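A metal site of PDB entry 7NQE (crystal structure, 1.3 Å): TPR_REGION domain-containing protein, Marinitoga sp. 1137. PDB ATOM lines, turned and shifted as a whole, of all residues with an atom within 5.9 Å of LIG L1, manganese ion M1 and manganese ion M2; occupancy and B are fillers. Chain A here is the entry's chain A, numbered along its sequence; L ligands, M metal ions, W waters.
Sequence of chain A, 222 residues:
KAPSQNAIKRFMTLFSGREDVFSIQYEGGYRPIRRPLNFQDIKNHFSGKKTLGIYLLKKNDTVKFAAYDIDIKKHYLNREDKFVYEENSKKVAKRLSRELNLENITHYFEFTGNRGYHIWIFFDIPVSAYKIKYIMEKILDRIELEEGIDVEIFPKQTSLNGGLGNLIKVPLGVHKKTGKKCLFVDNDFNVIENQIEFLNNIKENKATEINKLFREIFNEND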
ATOM      1  N   GLY A  28      35.598 -29.801  26.010  1.00  0.00           N
ATOM      2  CA  GLY A  28      35.245 -31.183  26.273  1.00  0.00           C
ATOM      3  C   GLY A  28      33.772 -31.499  26.145  1.00  0.00           C
ATOM      4  O   GLY A  28      33.383 -32.660  26.325  1.00  0.00           O
ATOM      5  N   GLY A  29      32.928 -30.511  25.846  1.00  0.00           N
ATOM      6  CA  GLY A  29      31.524 -30.810  25.626  1.00  0.00           C
ATOM      7  C   GLY A  29      30.649 -29.567  25.778  1.00  0.00           C
ATOM      8  O   GLY A  29      31.075 -28.454  25.461  1.00  0.00           O
ATOM      9  N   TYR A  30      29.428 -29.797  26.240  1.00  0.00           N
ATOM     10  CA  TYR A  30      28.484 -28.734  26.558  1.00  0.00           C
ATOM     11  C   TYR A  30      27.952 -28.965  27.956  1.00  0.00           C
ATOM     12  O   TYR A  30      27.665 -30.100  28.338  1.00  0.00           O
ATOM     13  CB  TYR A  30      27.320 -28.699  25.563  1.00  0.00           C
ATOM     14  CG  TYR A  30      27.664 -27.987  24.262  1.00  0.00           C
ATOM     15  CD1 TYR A  30      28.391 -28.631  23.270  1.00  0.00           C
ATOM     16  CD2 TYR A  30      27.257 -26.670  24.049  1.00  0.00           C
ATOM     17  CE1 TYR A  30      28.712 -27.975  22.080  1.00  0.00           C
ATOM     18  CE2 TYR A  30      27.562 -26.013  22.874  1.00  0.00           C
ATOM     19  CZ  TYR A  30      28.285 -26.660  21.899  1.00  0.00           C
ATOM     20  OH  TYR A  30      28.583 -25.985  20.749  1.00  0.00           O
ATOM     21  N   ASP A  69      22.193 -29.915   9.765  1.00  0.00           N
ATOM     22  CA  ASP A  69      23.569 -29.804  10.211  1.00  0.00           C
ATOM     23  C   ASP A  69      24.416 -30.548   9.177  1.00  0.00           C
ATOM     24  O   ASP A  69      24.369 -31.784   9.105  1.00  0.00           O
ATOM     25  CB  ASP A  69      23.688 -30.397  11.617  1.00  0.00           C
ATOM     26  CG  ASP A  69      25.100 -30.562  12.102  1.00  0.00           C
ATOM     27  OD1 ASP A  69      25.946 -29.649  11.895  1.00  0.00           O
ATOM     28  OD2 ASP A  69      25.380 -31.631  12.700  1.00  0.00           O
ATOM     29  N   ILE A  70      25.128 -29.792   8.355  1.00  0.00           N
ATOM     30  CA  ILE A  70      25.933 -30.334   7.257  1.00  0.00           C
ATOM     31  C   ILE A  70      27.384 -30.357   7.713  1.00  0.00           C
ATOM     32  O   ILE A  70      27.970 -29.299   7.975  1.00  0.00           O
ATOM     33  CB  ILE A  70      25.747 -29.486   5.987  1.00  0.00           C
ATOM     34  CG1 ILE A  70      24.277 -29.451   5.577  1.00  0.00           C
ATOM     35  CG2 ILE A  70      26.593 -30.033   4.848  1.00  0.00           C
ATOM     36  CD1 ILE A  70      23.930 -28.308   4.705  1.00  0.00           C
ATOM     37  N   ASP A  71      27.953 -31.566   7.807  1.00  0.00           N
ATOM     38  CA  ASP A  71      29.288 -31.769   8.348  1.00  0.00           C
ATOM     39  C   ASP A  71      30.212 -32.390   7.301  1.00  0.00           C
ATOM     40  O   ASP A  71      29.829 -33.332   6.602  1.00  0.00           O
ATOM     41  CB  ASP A  71      29.263 -32.748   9.529  1.00  0.00           C
ATOM     42  CG  ASP A  71      28.623 -32.153  10.755  1.00  0.00           C
ATOM     43  OD1 ASP A  71      28.490 -30.906  10.820  1.00  0.00           O
ATOM     44  OD2 ASP A  71      28.287 -32.936  11.678  1.00  0.00           O
ATOM     45  N   THR A 112      29.438 -22.714  10.473  1.00  0.00           N
ATOM     46  CA  THR A 112      29.415 -23.149  11.867  1.00  0.00           C
ATOM     47  C   THR A 112      30.748 -23.008  12.607  1.00  0.00           C
ATOM     48  O   THR A 112      30.869 -23.460  13.739  1.00  0.00           O
ATOM     49  CB  THR A 112      28.843 -24.578  11.988  1.00  0.00           C
ATOM     50  OG1 THR A 112      29.621 -25.505  11.221  1.00  0.00           O
ATOM     51  CG2 THR A 112      27.410 -24.619  11.495  1.00  0.00           C
ATOM     52  N   GLY A 113      31.745 -22.384  11.983  1.00  0.00           N
ATOM     53  CA  GLY A 113      33.002 -22.088  12.650  1.00  0.00           C
ATOM     54  C   GLY A 113      33.998 -23.210  12.689  1.00  0.00           C
ATOM     55  O   GLY A 113      35.017 -23.087  13.379  1.00  0.00           O
ATOM     56  N   ASN A 114      33.767 -24.301  11.952  1.00  0.00           N
ATOM     57  CA  ASN A 114      34.692 -25.431  12.006  1.00  0.00           C
ATOM     58  C   ASN A 114      34.620 -26.258  10.723  1.00  0.00           C
ATOM     59  O   ASN A 114      35.507 -26.145   9.877  1.00  0.00           O
ATOM     60  CB  ASN A 114      34.422 -26.292  13.249  1.00  0.00           C
ATOM     61  CG  ASN A 114      35.393 -27.460  13.377  1.00  0.00           C
ATOM     62  OD1 ASN A 114      36.541 -27.402  12.921  1.00  0.00           O
ATOM     63  ND2 ASN A 114      34.930 -28.542  14.002  1.00  0.00           N
ATOM     64  N   ARG A 115      33.589 -27.089  10.576  1.00  0.00           N
ATOM     65  CA  ARG A 115      33.590 -28.070   9.489  1.00  0.00           C
ATOM     66  C   ARG A 115      32.261 -28.195   8.747  1.00  0.00           C
ATOM     67  O   ARG A 115      31.976 -29.244   8.156  1.00  0.00           O
ATOM     68  CB  ARG A 115      34.081 -29.432   9.960  1.00  0.00           C
ATOM     69  CG  ARG A 115      33.383 -29.981  11.193  1.00  0.00           C
ATOM     70  CD  ARG A 115      32.165 -30.842  10.857  1.00  0.00           C
ATOM     71  NE  ARG A 115      31.605 -31.399  12.084  1.00  0.00           N
ATOM     72  CZ  ARG A 115      31.761 -32.655  12.457  1.00  0.00           C
ATOM     73  NH1 ARG A 115      32.458 -33.507  11.723  1.00  0.00           N
ATOM     74  NH2 ARG A 115      31.285 -33.053  13.636  1.00  0.00           N
ATOM     75  N   GLY A 116      31.454 -27.135   8.722  1.00  0.00           N
ATOM     76  CA  GLY A 116      30.306 -27.186   7.823  1.00  0.00           C
ATOM     77  C   GLY A 116      29.368 -26.016   7.981  1.00  0.00           C
ATOM     78  O   GLY A 116      29.786 -24.885   8.259  1.00  0.00           O
ATOM     79  N   TYR A 117      28.079 -26.311   7.789  1.00  0.00           N
ATOM     80  CA  TYR A 117      27.044 -25.297   7.732  1.00  0.00           C
ATOM     81  C   TYR A 117      25.825 -25.802   8.471  1.00  0.00           C
ATOM     82  O   TYR A 117      25.598 -27.021   8.553  1.00  0.00           O
ATOM     83  CB  TYR A 117      26.639 -24.998   6.273  1.00  0.00           C
ATOM     84  CG  TYR A 117      27.762 -24.309   5.546  1.00  0.00           C
ATOM     85  CD1 TYR A 117      27.939 -22.939   5.658  1.00  0.00           C
ATOM     86  CD2 TYR A 117      28.679 -25.046   4.806  1.00  0.00           C
ATOM     87  CE1 TYR A 117      29.003 -22.309   5.036  1.00  0.00           C
ATOM     88  CE2 TYR A 117      29.748 -24.423   4.189  1.00  0.00           C
ATOM     89  CZ  TYR A 117      29.903 -23.053   4.303  1.00  0.00           C
ATOM     90  OH  TYR A 117      30.958 -22.433   3.677  1.00  0.00           O
ATOM     91  N   HIS A 118      25.040 -24.866   8.994  1.00  0.00           N
ATOM     92  CA  HIS A 118      23.686 -25.150   9.423  1.00  0.00           C
ATOM     93  C   HIS A 118      22.754 -24.476   8.432  1.00  0.00           C
ATOM     94  O   HIS A 118      23.033 -23.364   7.962  1.00  0.00           O
ATOM     95  CB  HIS A 118      23.418 -24.559  10.813  1.00  0.00           C
ATOM     96  CG  HIS A 118      24.117 -25.280  11.913  1.00  0.00           C
ATOM     97  ND1 HIS A 118      24.452 -24.658  13.105  1.00  0.00           N
ATOM     98  CD2 HIS A 118      24.604 -26.545  12.013  1.00  0.00           C
ATOM     99  CE1 HIS A 118      25.108 -25.501  13.881  1.00  0.00           C
ATOM    100  NE2 HIS A 118      25.199 -26.657  13.247  1.00  0.00           N
ATOM    101  N   GLU A 152      22.768 -34.133   9.165  1.00  0.00           N
ATOM    102  CA  GLU A 152      21.916 -34.467  10.303  1.00  0.00           C
ATOM    103  C   GLU A 152      20.754 -33.500  10.387  1.00  0.00           C
ATOM    104  O   GLU A 152      20.805 -32.381   9.876  1.00  0.00           O
ATOM    105  CB  GLU A 152      22.734 -34.366  11.589  1.00  0.00           C
ATOM    106  CG  GLU A 152      23.841 -35.378  11.707  1.00  0.00           C
ATOM    107  CD  GLU A 152      24.823 -34.972  12.781  1.00  0.00           C
ATOM    108  OE1 GLU A 152      24.463 -35.082  13.963  1.00  0.00           O
ATOM    109  OE2 GLU A 152      25.940 -34.497  12.441  1.00  0.00           O
ATOM    110  N   PHE A 154      18.222 -31.602  13.138  1.00  0.00           N
ATOM    111  CA  PHE A 154      17.873 -31.211  14.492  1.00  0.00           C
ATOM    112  C   PHE A 154      16.477 -30.604  14.457  1.00  0.00           C
ATOM    113  O   PHE A 154      16.232 -29.689  13.656  1.00  0.00           O
ATOM    114  CB  PHE A 154      18.867 -30.164  15.019  1.00  0.00           C
ATOM    115  CG  PHE A 154      20.187 -30.738  15.432  1.00  0.00           C
ATOM    116  CD1 PHE A 154      21.169 -31.039  14.489  1.00  0.00           C
ATOM    117  CD2 PHE A 154      20.467 -30.961  16.774  1.00  0.00           C
ATOM    118  CE1 PHE A 154      22.402 -31.564  14.877  1.00  0.00           C
ATOM    119  CE2 PHE A 154      21.701 -31.478  17.169  1.00  0.00           C
ATOM    120  CZ  PHE A 154      22.668 -31.790  16.209  1.00  0.00           C
ATOM    121  N   LEU A 167      20.747 -30.322  21.876  1.00  0.00           N
ATOM    122  CA  LEU A 167      21.088 -28.908  21.847  1.00  0.00           C
ATOM    123  C   LEU A 167      21.875 -28.612  20.584  1.00  0.00           C
ATOM    124  O   LEU A 167      22.526 -29.495  20.009  1.00  0.00           O
ATOM    125  CB  LEU A 167      21.876 -28.471  23.105  1.00  0.00           C
ATOM    126  CG  LEU A 167      23.251 -29.121  23.266  1.00  0.00           C
ATOM    127  CD1 LEU A 167      24.363 -28.204  22.753  1.00  0.00           C
ATOM    128  CD2 LEU A 167      23.507 -29.489  24.723  1.00  0.00           C
ATOM    129  N   ILE A 168      21.823 -27.356  20.160  1.00  0.00           N
ATOM    130  CA  ILE A 168      22.535 -26.910  18.955  1.00  0.00           C
ATOM    131  C   ILE A 168      23.194 -25.571  19.246  1.00  0.00           C
ATOM    132  O   ILE A 168      22.602 -24.684  19.881  1.00  0.00           O
ATOM    133  CB  ILE A 168      21.633 -26.886  17.709  1.00  0.00           C
ATOM    134  CG1 ILE A 168      22.456 -26.616  16.455  1.00  0.00           C
ATOM    135  CG2 ILE A 168      20.472 -25.896  17.869  1.00  0.00           C
ATOM    136  CD1 ILE A 168      21.700 -26.960  15.189  1.00  0.00           C
ATOM    137  N   LYS A 169      24.458 -25.436  18.831  1.00  0.00           N
ATOM    138  CA  LYS A 169      25.165 -24.177  18.957  1.00  0.00           C
ATOM    139  C   LYS A 169      24.498 -23.166  18.034  1.00  0.00           C
ATOM    140  O   LYS A 169      24.270 -23.442  16.847  1.00  0.00           O
ATOM    141  CB  LYS A 169      26.624 -24.370  18.560  1.00  0.00           C
ATOM    142  CG  LYS A 169      27.434 -23.089  18.573  1.00  0.00           C
ATOM    143  CD  LYS A 169      28.944 -23.352  18.573  1.00  0.00           C
ATOM    144  CE  LYS A 169      29.395 -24.246  17.429  1.00  0.00           C
ATOM    145  NZ  LYS A 169      29.057 -23.771  16.058  1.00  0.00           N
ATOM    146  N   VAL A 170      24.193 -21.984  18.568  1.00  0.00           N
ATOM    147  CA  VAL A 170      23.476 -20.968  17.797  1.00  0.00           C
ATOM    148  C   VAL A 170      24.456 -19.956  17.191  1.00  0.00           C
ATOM    149  O   VAL A 170      25.582 -19.805  17.703  1.00  0.00           O
ATOM    150  CB  VAL A 170      22.340 -20.322  18.618  1.00  0.00           C
ATOM    151  CG1 VAL A 170      21.211 -21.328  18.787  1.00  0.00           C
ATOM    152  CG2 VAL A 170      22.848 -19.833  19.963  1.00  0.00           C
ATOM    153  N   HIS A 175      33.158 -20.687  17.990  1.00  0.00           N
ATOM    154  CA  HIS A 175      33.304 -22.126  18.164  1.00  0.00           C
ATOM    155  C   HIS A 175      34.562 -22.389  18.979  1.00  0.00           C
ATOM    156  O   HIS A 175      35.669 -22.070  18.541  1.00  0.00           O
ATOM    157  CB  HIS A 175      33.433 -22.792  16.790  1.00  0.00           C
ATOM    158  CG  HIS A 175      33.164 -24.268  16.775  1.00  0.00           C
ATOM    159  ND1 HIS A 175      33.519 -25.105  17.811  1.00  0.00           N
ATOM    160  CD2 HIS A 175      32.583 -25.046  15.839  1.00  0.00           C
ATOM    161  CE1 HIS A 175      33.157 -26.343  17.519  1.00  0.00           C
ATOM    162  NE2 HIS A 175      32.590 -26.337  16.315  1.00  0.00           N
ATOM    163  N   LYS A 177      36.207 -24.989  19.517  1.00  0.00           N
ATOM    164  CA  LYS A 177      37.185 -25.918  18.941  1.00  0.00           C
ATOM    165  C   LYS A 177      38.217 -25.192  18.091  1.00  0.00           C
ATOM    166  O   LYS A 177      39.355 -25.663  17.964  1.00  0.00           O
ATOM    167  CB  LYS A 177      36.483 -26.982  18.098  1.00  0.00           C
ATOM    168  CG  LYS A 177      35.920 -28.164  18.884  1.00  0.00           C
ATOM    169  CD  LYS A 177      35.315 -29.218  17.953  1.00  0.00           C
ATOM    170  CE  LYS A 177      34.748 -30.387  18.741  1.00  0.00           C
ATOM    171  NZ  LYS A 177      34.185 -31.431  17.837  1.00  0.00           N
HETATM  172  P1  LIG L   1      30.955 -28.037  13.460  1.00  0.00           P
HETATM  173  O1  LIG L   1      31.389 -27.030  12.395  1.00  0.00           O
HETATM  174  O2  LIG L   1      32.042 -28.424  14.383  1.00  0.00           O
HETATM  175  O3  LIG L   1      30.136 -29.235  12.840  1.00  0.00           O
HETATM  176  O4  LIG L   1      29.935 -27.121  14.400  1.00  0.00           O
HETATM  177  P2  LIG L   1      28.460 -27.712  14.982  1.00  0.00           P
HETATM  178  O5  LIG L   1      27.500 -28.060  13.850  1.00  0.00           O
HETATM  179  O6  LIG L   1      28.008 -26.772  16.109  1.00  0.00           O
HETATM  180  O7  LIG L   1      28.965 -29.169  15.696  1.00  0.00           O
HETATM  181  P3  LIG L   1      28.551 -30.707  15.406  1.00  0.00           P
HETATM  182  O8  LIG L   1      29.726 -31.529  15.835  1.00  0.00           O
HETATM  183  O9  LIG L   1      28.030 -30.935  14.089  1.00  0.00           O
HETATM  184  O10 LIG L   1      27.337 -30.955  16.496  1.00  0.00           O
HETATM  185  C1  LIG L   1      26.037 -30.372  16.267  1.00  0.00           C
HETATM  186  C2  LIG L   1      25.483 -29.889  17.467  1.00  0.00           C
HETATM  187  O11 LIG L   1      25.486 -31.003  18.524  1.00  0.00           O
HETATM  188  C3  LIG L   1      26.294 -28.767  18.162  1.00  0.00           C
HETATM  189  O12 LIG L   1      25.940 -27.491  17.566  1.00  0.00           O
HETATM  190  C4  LIG L   1      25.956 -28.866  19.457  1.00  0.00           C
HETATM  191  C5  LIG L   1      25.737 -30.471  19.685  1.00  0.00           C
HETATM  192  N1  LIG L   1      26.898 -31.045  20.337  1.00  0.00           N
HETATM  193  C6  LIG L   1      28.032 -31.076  19.620  1.00  0.00           C
HETATM  194  N2  LIG L   1      28.999 -31.600  20.422  1.00  0.00           N
HETATM  195  C7  LIG L   1      28.452 -31.872  21.597  1.00  0.00           C
HETATM  196  C8  LIG L   1      29.002 -32.482  22.896  1.00  0.00           C
HETATM  197  O13 LIG L   1      30.151 -32.801  22.998  1.00  0.00           O
HETATM  198  N3  LIG L   1      28.126 -32.623  23.977  1.00  0.00           N
HETATM  199  C9  LIG L   1      26.739 -32.251  23.875  1.00  0.00           C
HETATM  200  N4  LIG L   1      25.861 -32.405  24.996  1.00  0.00           N
HETATM  201  N5  LIG L   1      26.212 -31.686  22.645  1.00  0.00           N
HETATM  202  C10 LIG L   1      27.141 -31.526  21.540  1.00  0.00           C
HETATM  203  C1  LG2 L   2      26.742 -34.170  16.097  1.00  0.00           C
HETATM  204  O1  LG2 L   2      25.947 -33.408  15.176  1.00  0.00           O
HETATM  205  C2  LG2 L   2      27.746 -35.019  15.331  1.00  0.00           C
HETATM  206  O2  LG2 L   2      28.432 -34.218  14.357  1.00  0.00           O
HETATM  207 MN    MN M   1      27.021 -32.804  13.326  1.00  0.00          MN
HETATM  208 MN    MN M   2      28.052 -29.486  12.318  1.00  0.00          MN
HETATM  209  O   HOH W   1      32.103 -30.231  16.338  1.00  0.00           O
HETATM  210  O   HOH W   2      31.879 -30.802  21.163  1.00  0.00           O
HETATM  211  O   HOH W   3      28.173 -27.932  10.702  1.00  0.00           O
HETATM  212  O   HOH W   4      31.874 -32.680  19.145  1.00  0.00           O
HETATM  213  O   HOH W   5      30.367 -33.603  17.450  1.00  0.00           O
HETATM  214  O   HOH W   6      23.002 -33.437  24.269  1.00  0.00           O
HETATM  215  O   HOH W   7      29.402 -27.464  18.604  1.00  0.00           O
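Water W3 lies within hydrogen-bond range of OG1 of Thr 112 (2.9 Å), O of Ile 70 (3.1 Å) and N of Tyr 117 (3.3 Å). Water W1 lies within hydrogen-bond range of O2 of LIG L1 and NZ of Lys 177. Water W7 bridges OH of Tyr 30 and O6 of LIG L1. Water W4 lies within hydrogen-bond range of the side-chain amino group of Lys 177 (2.9 Å) and a nitrogen (N2) of LIG L1 (3.3 Å).
Manganese ion M2 is bound by the side-chain carboxylate (OD1) of Asp 71 (2.1 Å), the side-chain carboxylate (OD1) of Asp 69 (2.2 Å), an oxygen (O3) of LIG L1 (2.2 Å), an oxygen (O5) of LIG L1 (2.2 Å), water W3 (2.2 Å) and an oxygen (O9) of LIG L1 (2.3 Å). Manganese ion M2 has six donor atoms within binding distance.
NE of Arg 115 lies close to OD1 of Asp 71 (3.4 Å). The side-chain carboxylate of Asp 69 lies close to a ring nitrogen (NE2) of His 118. The side-chain amino group (NZ) of Lys 169 is in hydrogen-bond range of the backbone carbonyl oxygen (O) of Thr 112 (3.0 Å). OG1 of Thr 112 is in hydrogen-bond range of O of Gly 116, 3.0 Å away. A ring nitrogen (ND1) of His 175 lies close to the backbone NH (N) of Lys 177.
Gly 29 touches LIG L1. Tyr 30 touches LIG L1. Gly 116 touches LIG L1 (N to O1, 3.7 Å). CZ of Phe 154 touches C2 of LIG L1, 3.6 Å away. Leu 167 touches LIG L1. CA of Ile 168 touches O12 of LIG L1 (3.7 Å). Within 4 Å of LIG L1: Gly 29, Tyr 30, Asp 69, Asp 71, Thr 112, Asn 114, Arg 115, Gly 116, His 118, Phe 154, Leu 167, Ile 168, Lys 169 and His 175. The nearest printed residue that does not touch LIG L1 is Glu 152 (4.4 Å).
Within 4 Å of manganese ion M1: Asp 69, Asp 71 and Glu 152.
Manganese ion M1 is bound by the side-chain carboxylate of Asp 71, the side-chain carboxylate of Asp 69, the side-chain carboxylate of Glu 152, an oxygen (O1) of LG2 L2, an oxygen (O2) of LG2 L2 and an oxygen (O9) of LIG L1.
OG1 of Thr 112 is in hydrogen-bond range of O1 of LIG L1. N of Arg 115 is in hydrogen-bond range of O1 of LIG L1. O8 of LIG L1 lies within salt-bridge range of NH2 of Arg 115. NE2 of His 118 sits close to O5 of LIG L1. N of Lys 169 lies within hydrogen-bond range of O12 of LIG L1, 2.8 Å away. O6 of LIG L1 lies within salt-bridge range of NZ of Lys 169 (3.2 Å). A ring nitrogen (NE2) of His 175 lies within hydrogen-bond range of an oxygen (O2) of LIG L1. O2 of LIG L1 is in hydrogen-bond range of ND2 of Asn 114, 2.9 Å away.
The nearest printed residue that does not touch manganese ion M2 is Arg 115 (4.04 Å).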
